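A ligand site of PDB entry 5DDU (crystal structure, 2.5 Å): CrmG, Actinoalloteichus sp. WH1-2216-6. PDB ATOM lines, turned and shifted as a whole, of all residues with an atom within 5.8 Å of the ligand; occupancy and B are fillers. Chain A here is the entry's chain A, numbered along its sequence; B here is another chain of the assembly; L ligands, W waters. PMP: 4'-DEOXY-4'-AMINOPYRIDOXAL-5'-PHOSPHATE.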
ATOM      1  N   PHE A  55      29.541   0.225   2.972  1.00  0.00           N
ATOM      2  CA  PHE A  55      29.105   1.443   2.305  1.00  0.00           C
ATOM      3  C   PHE A  55      27.668   1.826   2.680  1.00  0.00           C
ATOM      4  O   PHE A  55      26.888   2.235   1.827  1.00  0.00           O
ATOM      5  CB  PHE A  55      29.210   1.291   0.772  1.00  0.00           C
ATOM      6  CG  PHE A  55      30.613   1.119   0.271  1.00  0.00           C
ATOM      7  CD1 PHE A  55      31.583   2.092   0.539  1.00  0.00           C
ATOM      8  CD2 PHE A  55      30.973   0.010  -0.444  1.00  0.00           C
ATOM      9  CE1 PHE A  55      32.884   1.946   0.097  1.00  0.00           C
ATOM     10  CE2 PHE A  55      32.287  -0.151  -0.895  1.00  0.00           C
ATOM     11  CZ  PHE A  55      33.238   0.814  -0.620  1.00  0.00           C
ATOM     12  N   ASN A 118      17.990  -8.876  -6.391  1.00  0.00           N
ATOM     13  CA  ASN A 118      19.141  -9.360  -5.654  1.00  0.00           C
ATOM     14  C   ASN A 118      20.261  -8.293  -5.415  1.00  0.00           C
ATOM     15  O   ASN A 118      21.211  -8.548  -4.693  1.00  0.00           O
ATOM     16  CB  ASN A 118      19.739 -10.546  -6.387  1.00  0.00           C
ATOM     17  CG  ASN A 118      18.694 -11.567  -6.748  1.00  0.00           C
ATOM     18  OD1 ASN A 118      18.070 -12.190  -5.862  1.00  0.00           O
ATOM     19  ND2 ASN A 118      18.476 -11.751  -8.051  1.00  0.00           N
ATOM     20  N   SER A 119      20.123  -7.125  -6.015  1.00  0.00           N
ATOM     21  CA  SER A 119      21.057  -6.049  -5.761  1.00  0.00           C
ATOM     22  C   SER A 119      20.436  -4.746  -6.146  1.00  0.00           C
ATOM     23  O   SER A 119      19.348  -4.721  -6.731  1.00  0.00           O
ATOM     24  CB  SER A 119      22.341  -6.264  -6.535  1.00  0.00           C
ATOM     25  OG  SER A 119      22.056  -6.304  -7.920  1.00  0.00           O
ATOM     26  N   GLY A 120      21.103  -3.658  -5.785  1.00  0.00           N
ATOM     27  CA  GLY A 120      20.611  -2.330  -6.076  1.00  0.00           C
ATOM     28  C   GLY A 120      20.513  -2.087  -7.569  1.00  0.00           C
ATOM     29  O   GLY A 120      19.552  -1.488  -8.050  1.00  0.00           O
ATOM     30  N   ALA A 121      21.527  -2.544  -8.282  1.00  0.00           N
ATOM     31  CA  ALA A 121      21.577  -2.372  -9.709  1.00  0.00           C
ATOM     32  C   ALA A 121      20.433  -3.112 -10.376  1.00  0.00           C
ATOM     33  O   ALA A 121      19.814  -2.588 -11.313  1.00  0.00           O
ATOM     34  CB  ALA A 121      22.925  -2.856 -10.254  1.00  0.00           C
ATOM     35  N   GLU A 122      20.142  -4.324  -9.892  1.00  0.00           N
ATOM     36  CA  GLU A 122      19.042  -5.106 -10.421  1.00  0.00           C
ATOM     37  C   GLU A 122      17.705  -4.377 -10.200  1.00  0.00           C
ATOM     38  O   GLU A 122      16.827  -4.410 -11.064  1.00  0.00           O
ATOM     39  CB  GLU A 122      18.975  -6.482  -9.752  1.00  0.00           C
ATOM     40  CG  GLU A 122      20.045  -7.475 -10.219  1.00  0.00           C
ATOM     41  CD  GLU A 122      19.711  -8.914  -9.846  1.00  0.00           C
ATOM     42  OE1 GLU A 122      18.922  -9.136  -8.893  1.00  0.00           O
ATOM     43  OE2 GLU A 122      20.237  -9.828 -10.513  1.00  0.00           O
ATOM     44  N   ASN A 124      17.232  -1.042  -9.677  1.00  0.00           N
ATOM     45  CA  ASN A 124      17.230   0.101 -10.586  1.00  0.00           C
ATOM     46  C   ASN A 124      16.970  -0.306 -12.008  1.00  0.00           C
ATOM     47  O   ASN A 124      16.358   0.425 -12.744  1.00  0.00           O
ATOM     48  CB  ASN A 124      18.523   0.883 -10.475  1.00  0.00           C
ATOM     49  CG  ASN A 124      18.552   1.754  -9.260  1.00  0.00           C
ATOM     50  OD1 ASN A 124      17.532   1.998  -8.626  1.00  0.00           O
ATOM     51  ND2 ASN A 124      19.729   2.239  -8.900  1.00  0.00           N
ATOM     52  N   PHE A 207      25.539   7.693  -8.873  1.00  0.00           N
ATOM     53  CA  PHE A 207      26.011   6.323  -8.729  1.00  0.00           C
ATOM     54  C   PHE A 207      24.757   5.447  -8.561  1.00  0.00           C
ATOM     55  O   PHE A 207      24.112   5.462  -7.515  1.00  0.00           O
ATOM     56  CB  PHE A 207      26.927   6.220  -7.507  1.00  0.00           C
ATOM     57  CG  PHE A 207      27.710   4.909  -7.409  1.00  0.00           C
ATOM     58  CD1 PHE A 207      27.384   3.793  -8.179  1.00  0.00           C
ATOM     59  CD2 PHE A 207      28.781   4.798  -6.496  1.00  0.00           C
ATOM     60  CE1 PHE A 207      28.105   2.603  -8.074  1.00  0.00           C
ATOM     61  CE2 PHE A 207      29.501   3.603  -6.382  1.00  0.00           C
ATOM     62  CZ  PHE A 207      29.163   2.503  -7.166  1.00  0.00           C
ATOM     63  N   HIS A 208      24.407   4.695  -9.613  1.00  0.00           N
ATOM     64  CA  HIS A 208      23.148   3.895  -9.632  1.00  0.00           C
ATOM     65  C   HIS A 208      23.415   2.403  -9.884  1.00  0.00           C
ATOM     66  O   HIS A 208      22.472   1.595  -9.995  1.00  0.00           O
ATOM     67  CB  HIS A 208      22.193   4.447 -10.716  1.00  0.00           C
ATOM     68  CG  HIS A 208      21.648   5.795 -10.396  1.00  0.00           C
ATOM     69  ND1 HIS A 208      20.902   6.049  -9.256  1.00  0.00           N
ATOM     70  CD2 HIS A 208      21.755   6.983 -11.041  1.00  0.00           C
ATOM     71  CE1 HIS A 208      20.582   7.328  -9.231  1.00  0.00           C
ATOM     72  NE2 HIS A 208      21.077   7.914 -10.298  1.00  0.00           N
ATOM     73  N   GLY A 209      24.688   2.037  -9.968  1.00  0.00           N
ATOM     74  CA  GLY A 209      25.079   0.628 -10.175  1.00  0.00           C
ATOM     75  C   GLY A 209      26.002   0.496 -11.362  1.00  0.00           C
ATOM     76  O   GLY A 209      26.191   1.464 -12.146  1.00  0.00           O
ATOM     77  N   LYS A 210      26.585  -0.700 -11.498  1.00  0.00           N
ATOM     78  CA  LYS A 210      27.732  -0.890 -12.374  1.00  0.00           C
ATOM     79  C   LYS A 210      27.515  -2.029 -13.382  1.00  0.00           C
ATOM     80  O   LYS A 210      28.459  -2.495 -13.999  1.00  0.00           O
ATOM     81  CB  LYS A 210      28.990  -1.159 -11.544  1.00  0.00           C
ATOM     82  CG  LYS A 210      29.216  -0.139 -10.418  1.00  0.00           C
ATOM     83  CD  LYS A 210      30.529   0.638 -10.593  1.00  0.00           C
ATOM     84  CE  LYS A 210      31.742  -0.282 -10.464  1.00  0.00           C
ATOM     85  NZ  LYS A 210      32.857   0.334  -9.705  1.00  0.00           N
ATOM     86  N   GLU A 282      19.300  10.350  -6.467  1.00  0.00           N
ATOM     87  CA  GLU A 282      19.595   9.916  -5.097  1.00  0.00           C
ATOM     88  C   GLU A 282      19.311  11.042  -4.145  1.00  0.00           C
ATOM     89  O   GLU A 282      19.825  12.141  -4.324  1.00  0.00           O
ATOM     90  CB  GLU A 282      21.089   9.560  -4.958  1.00  0.00           C
ATOM     91  CG  GLU A 282      21.634   8.529  -5.937  1.00  0.00           C
ATOM     92  CD  GLU A 282      23.148   8.465  -5.881  1.00  0.00           C
ATOM     93  OE1 GLU A 282      23.808   8.909  -6.829  1.00  0.00           O
ATOM     94  OE2 GLU A 282      23.693   7.953  -4.846  1.00  0.00           O
ATOM     95  N   VAL A 284      20.435  11.519  -1.261  1.00  0.00           N
ATOM     96  CA  VAL A 284      21.746  11.948  -0.828  1.00  0.00           C
ATOM     97  C   VAL A 284      22.733  11.258  -1.700  1.00  0.00           C
ATOM     98  O   VAL A 284      22.682  10.027  -1.860  1.00  0.00           O
ATOM     99  CB  VAL A 284      21.998  11.586   0.648  1.00  0.00           C
ATOM    100  CG1 VAL A 284      23.233  12.296   1.173  1.00  0.00           C
ATOM    101  CG2 VAL A 284      20.782  11.956   1.506  1.00  0.00           C
ATOM    102  N   GLY A 286      25.819   9.728  -3.199  1.00  0.00           N
ATOM    103  CA  GLY A 286      27.027   9.063  -2.729  1.00  0.00           C
ATOM    104  C   GLY A 286      28.246   9.333  -3.573  1.00  0.00           C
ATOM    105  O   GLY A 286      29.319   9.674  -3.053  1.00  0.00           O
ATOM    106  N   ASP A 315      16.244   6.715  -6.031  1.00  0.00           N
ATOM    107  CA  ASP A 315      17.161   5.608  -5.676  1.00  0.00           C
ATOM    108  C   ASP A 315      17.533   5.752  -4.212  1.00  0.00           C
ATOM    109  O   ASP A 315      18.331   6.603  -3.852  1.00  0.00           O
ATOM    110  CB  ASP A 315      18.422   5.664  -6.577  1.00  0.00           C
ATOM    111  CG  ASP A 315      19.476   4.549  -6.258  1.00  0.00           C
ATOM    112  OD1 ASP A 315      19.418   3.942  -5.144  1.00  0.00           O
ATOM    113  OD2 ASP A 315      20.388   4.309  -7.140  1.00  0.00           O
ATOM    114  N   VAL A 317      18.695   3.071  -2.405  1.00  0.00           N
ATOM    115  CA  VAL A 317      19.596   1.993  -2.045  1.00  0.00           C
ATOM    116  C   VAL A 317      20.431   2.347  -0.783  1.00  0.00           C
ATOM    117  O   VAL A 317      20.508   1.535   0.144  1.00  0.00           O
ATOM    118  CB  VAL A 317      20.522   1.647  -3.199  1.00  0.00           C
ATOM    119  CG1 VAL A 317      21.707   0.860  -2.704  1.00  0.00           C
ATOM    120  CG2 VAL A 317      19.760   0.870  -4.267  1.00  0.00           C
ATOM    121  N   GLN A 318      21.032   3.538  -0.753  1.00  0.00           N
ATOM    122  CA  GLN A 318      21.842   3.981   0.398  1.00  0.00           C
ATOM    123  C   GLN A 318      21.035   4.703   1.459  1.00  0.00           C
ATOM    124  O   GLN A 318      21.136   4.385   2.639  1.00  0.00           O
ATOM    125  CB  GLN A 318      22.947   4.887  -0.062  1.00  0.00           C
ATOM    126  CG  GLN A 318      24.264   4.205  -0.269  1.00  0.00           C
ATOM    127  CD  GLN A 318      25.415   5.187  -0.291  1.00  0.00           C
ATOM    128  OE1 GLN A 318      25.838   5.693   0.755  1.00  0.00           O
ATOM    129  NE2 GLN A 318      25.920   5.482  -1.478  1.00  0.00           N
ATOM    130  N   ALA A 343      17.761  -1.314  -1.221  1.00  0.00           N
ATOM    131  CA  ALA A 343      18.620  -2.481  -1.102  1.00  0.00           C
ATOM    132  C   ALA A 343      19.430  -2.450   0.237  1.00  0.00           C
ATOM    133  O   ALA A 343      18.911  -2.110   1.311  1.00  0.00           O
ATOM    134  CB  ALA A 343      19.556  -2.547  -2.321  1.00  0.00           C
ATOM    135  N   LYS A 344      20.711  -2.791   0.132  1.00  0.00           N
ATOM    136  CA  LYS A 344      21.672  -2.671   1.236  1.00  0.00           C
ATOM    137  C   LYS A 344      21.196  -3.201   2.639  1.00  0.00           C
ATOM    138  O   LYS A 344      21.384  -4.446   2.972  1.00  0.00           O
ATOM    139  CB  LYS A 344      22.229  -1.248   1.311  1.00  0.00           C
ATOM    140  CG  LYS A 344      23.473  -1.109   0.442  1.00  0.00           C
ATOM    141  CD  LYS A 344      24.105   0.265   0.467  1.00  0.00           C
ATOM    142  CE  LYS A 344      24.925   0.489  -0.802  1.00  0.00           C
ATOM    143  NZ  LYS A 344      26.180   1.229  -0.543  1.00  0.00           N
ATOM    144  N   ASN B 118      26.232 -11.449  -7.864  1.00  0.00           N
ATOM    145  CA  ASN B 118      25.073 -11.813  -7.058  1.00  0.00           C
ATOM    146  C   ASN B 118      23.990 -12.623  -7.806  1.00  0.00           C
ATOM    147  O   ASN B 118      23.041 -13.083  -7.209  1.00  0.00           O
ATOM    148  CB  ASN B 118      24.464 -10.549  -6.454  1.00  0.00           C
ATOM    149  CG  ASN B 118      25.513  -9.670  -5.782  1.00  0.00           C
ATOM    150  OD1 ASN B 118      26.122 -10.062  -4.774  1.00  0.00           O
ATOM    151  ND2 ASN B 118      25.733  -8.487  -6.327  1.00  0.00           N
ATOM    152  N   GLU B 122      24.146 -11.028 -13.587  1.00  0.00           N
ATOM    153  CA  GLU B 122      25.270 -10.126 -13.209  1.00  0.00           C
ATOM    154  C   GLU B 122      26.602 -10.729 -13.691  1.00  0.00           C
ATOM    155  O   GLU B 122      27.493 -10.009 -14.150  1.00  0.00           O
ATOM    156  CB  GLU B 122      25.315  -9.944 -11.693  1.00  0.00           C
ATOM    157  CG  GLU B 122      24.207  -9.028 -11.120  1.00  0.00           C
ATOM    158  CD  GLU B 122      24.508  -8.568  -9.692  1.00  0.00           C
ATOM    159  OE1 GLU B 122      25.325  -9.223  -8.993  1.00  0.00           O
ATOM    160  OE2 GLU B 122      23.947  -7.538  -9.281  1.00  0.00           O
ATOM    161  N   SER B 372      32.856  -3.505  -9.719  1.00  0.00           N
ATOM    162  CA  SER B 372      32.650  -3.776  -8.300  1.00  0.00           C
ATOM    163  C   SER B 372      31.133  -3.824  -8.020  1.00  0.00           C
ATOM    164  O   SER B 372      30.325  -3.432  -8.871  1.00  0.00           O
ATOM    165  CB  SER B 372      33.286  -2.667  -7.452  1.00  0.00           C
ATOM    166  OG  SER B 372      32.599  -1.466  -7.608  1.00  0.00           O
ATOM    167  N   SER B 373      30.762  -4.260  -6.815  1.00  0.00           N
ATOM    168  CA  SER B 373      29.341  -4.401  -6.426  1.00  0.00           C
ATOM    169  C   SER B 373      29.298  -4.439  -4.881  1.00  0.00           C
ATOM    170  O   SER B 373      30.243  -4.901  -4.270  1.00  0.00           O
ATOM    171  CB  SER B 373      28.783  -5.706  -7.004  1.00  0.00           C
ATOM    172  OG  SER B 373      27.416  -5.892  -6.660  1.00  0.00           O
ATOM    173  N   THR B 374      28.216  -3.941  -4.271  1.00  0.00           N
ATOM    174  CA  THR B 374      28.146  -3.850  -2.782  1.00  0.00           C
ATOM    175  C   THR B 374      28.165  -5.244  -2.133  1.00  0.00           C
ATOM    176  O   THR B 374      28.968  -5.509  -1.237  1.00  0.00           O
ATOM    177  CB  THR B 374      26.881  -3.086  -2.315  1.00  0.00           C
ATOM    178  OG1 THR B 374      27.010  -1.710  -2.677  1.00  0.00           O
ATOM    179  CG2 THR B 374      26.719  -3.179  -0.823  1.00  0.00           C
ATOM    180  N   PHE B 375      27.294  -6.132  -2.627  1.00  0.00           N
ATOM    181  CA  PHE B 375      27.044  -7.407  -2.029  1.00  0.00           C
ATOM    182  C   PHE B 375      28.013  -8.502  -2.540  1.00  0.00           C
ATOM    183  O   PHE B 375      28.089  -9.598  -1.947  1.00  0.00           O
ATOM    184  CB  PHE B 375      25.614  -7.858  -2.361  1.00  0.00           C
ATOM    185  CG  PHE B 375      24.541  -7.163  -1.555  1.00  0.00           C
ATOM    186  CD1 PHE B 375      24.778  -6.735  -0.247  1.00  0.00           C
ATOM    187  CD2 PHE B 375      23.279  -6.978  -2.101  1.00  0.00           C
ATOM    188  CE1 PHE B 375      23.779  -6.130   0.478  1.00  0.00           C
ATOM    189  CE2 PHE B 375      22.288  -6.363  -1.371  1.00  0.00           C
ATOM    190  CZ  PHE B 375      22.539  -5.946  -0.080  1.00  0.00           C
HETATM  191  N1  PMP L   1      22.522   3.102  -5.830  1.00  0.00           N
HETATM  192  C2  PMP L   1      23.301   3.555  -4.799  1.00  0.00           C
HETATM  193  C2A PMP L   1      22.984   4.863  -4.135  1.00  0.00           C
HETATM  194  C3  PMP L   1      24.386   2.789  -4.361  1.00  0.00           C
HETATM  195  O3  PMP L   1      25.185   3.196  -3.343  1.00  0.00           O
HETATM  196  C4  PMP L   1      24.655   1.607  -4.958  1.00  0.00           C
HETATM  197  C4A PMP L   1      25.836   0.838  -4.453  1.00  0.00           C
HETATM  198  N4A PMP L   1      27.019   1.692  -4.588  1.00  0.00           N
HETATM  199  C5  PMP L   1      23.874   1.167  -5.994  1.00  0.00           C
HETATM  200  C6  PMP L   1      22.798   1.931  -6.421  1.00  0.00           C
HETATM  201  C5A PMP L   1      24.173  -0.162  -6.646  1.00  0.00           C
HETATM  202  O4P PMP L   1      23.866  -1.151  -5.658  1.00  0.00           O
HETATM  203  P   PMP L   1      24.510  -2.660  -5.678  1.00  0.00           P
HETATM  204  O1P PMP L   1      23.765  -3.538  -4.668  1.00  0.00           O
HETATM  205  O2P PMP L   1      24.314  -3.202  -7.104  1.00  0.00           O
HETATM  206  O3P PMP L   1      25.928  -2.529  -5.291  1.00  0.00           O
HETATM  207  O   HOH W   1      25.715   6.037  -4.291  1.00  0.00           O
HETATM  208  O   HOH W   2      22.594   7.368  -2.196  1.00  0.00           O
HETATM  209  O   HOH W   3      25.402  -5.589  -4.733  1.00  0.00           O
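OD2 of Asp 315 is in hydrogen-bond range of N1 of the ligand (2.8 Å). The backbone NH (N) of Thr 374 of chain B sits at hydrogen-bond distance from an oxygen (O3P) of the ligand, 2.9 Å away. An oxygen (O3P) of the ligand sits at hydrogen-bond distance from the side-chain hydroxyl (OG1) of Thr 374 of chain B (2.9 Å). N of Gly 120 lies within hydrogen-bond range of O1P of the ligand (2.9 Å). NE2 of Gln 318 is in hydrogen-bond range of O3 of the ligand (3.0 Å). The backbone NH of Ala 121 is in hydrogen-bond range of an oxygen (O2P) of the ligand, at 3.1 Å.
OD2 of Asp 315 lies within hydrogen-bond range of ND1 of His 208 (2.8 Å). The side-chain carboxylate (OD1) of Asp 315 sits at hydrogen-bond distance from the backbone NH (N) of Val 317 (3.0 Å). The side-chain carboxylate of Asp 315 is in hydrogen-bond range of the side-chain amide nitrogen of Asn 124 (2.8 Å). The side-chain carboxylate (OE1) of Glu 282 is in hydrogen-bond range of the backbone NH (N) of Phe 207. The side-chain carboxylate (OE2) of Glu 282 lies within hydrogen-bond range of the backbone NH (N) of Gly 286 (3.2 Å). The backbone carbonyl oxygen (O) of Phe 55 sits at hydrogen-bond distance from the side-chain amino group (NZ) of Lys 344 (2.7 Å). The side-chain hydroxyl (OG) of Ser 119 is in hydrogen-bond range of the side-chain carboxylate (OE2) of Glu 122 of chain B, 2.6 Å away. ND2 of Asn 118 of chain B lies within hydrogen-bond range of OG of Ser 373 of chain B (3.1 Å).
O of Phe 207 lies close to N1 of the ligand, 3.3 Å away. Ser 119 touches the ligand (CB to O1P, 3.6 Å). ND2 of Asn 124 touches C6 of the ligand, 3.96 Å away. His 208 touches the ligand. Gly 209 touches the ligand. OE2 of Glu 282 touches C2A of the ligand (3.2 Å). Val 317 touches the ligand (CB to N1, 3.6 Å). NZ of Lys 344 touches O3 of the ligand, 3.6 Å away. Ser 373 of chain B touches the ligand. Hydrophobic or aromatic side chains within 4 Å of the ligand: Ala 121, Phe 207 and Val 317. Of the 25 residues printed, 14 come within 4 Å of the ligand. The nearest printed residue that does not touch the ligand is Phe 375 of chain B (4.3 Å).
Water W1 lies within hydrogen-bond range of the side-chain carboxylate (OE2) of Glu 282, the side-chain amide nitrogen (NE2) of Gln 318 and an oxygen (O3) of the ligand. Water W2 lies within hydrogen-bond range of O of Val 284 (2.7 Å) and OE2 of Glu 282 (2.9 Å).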
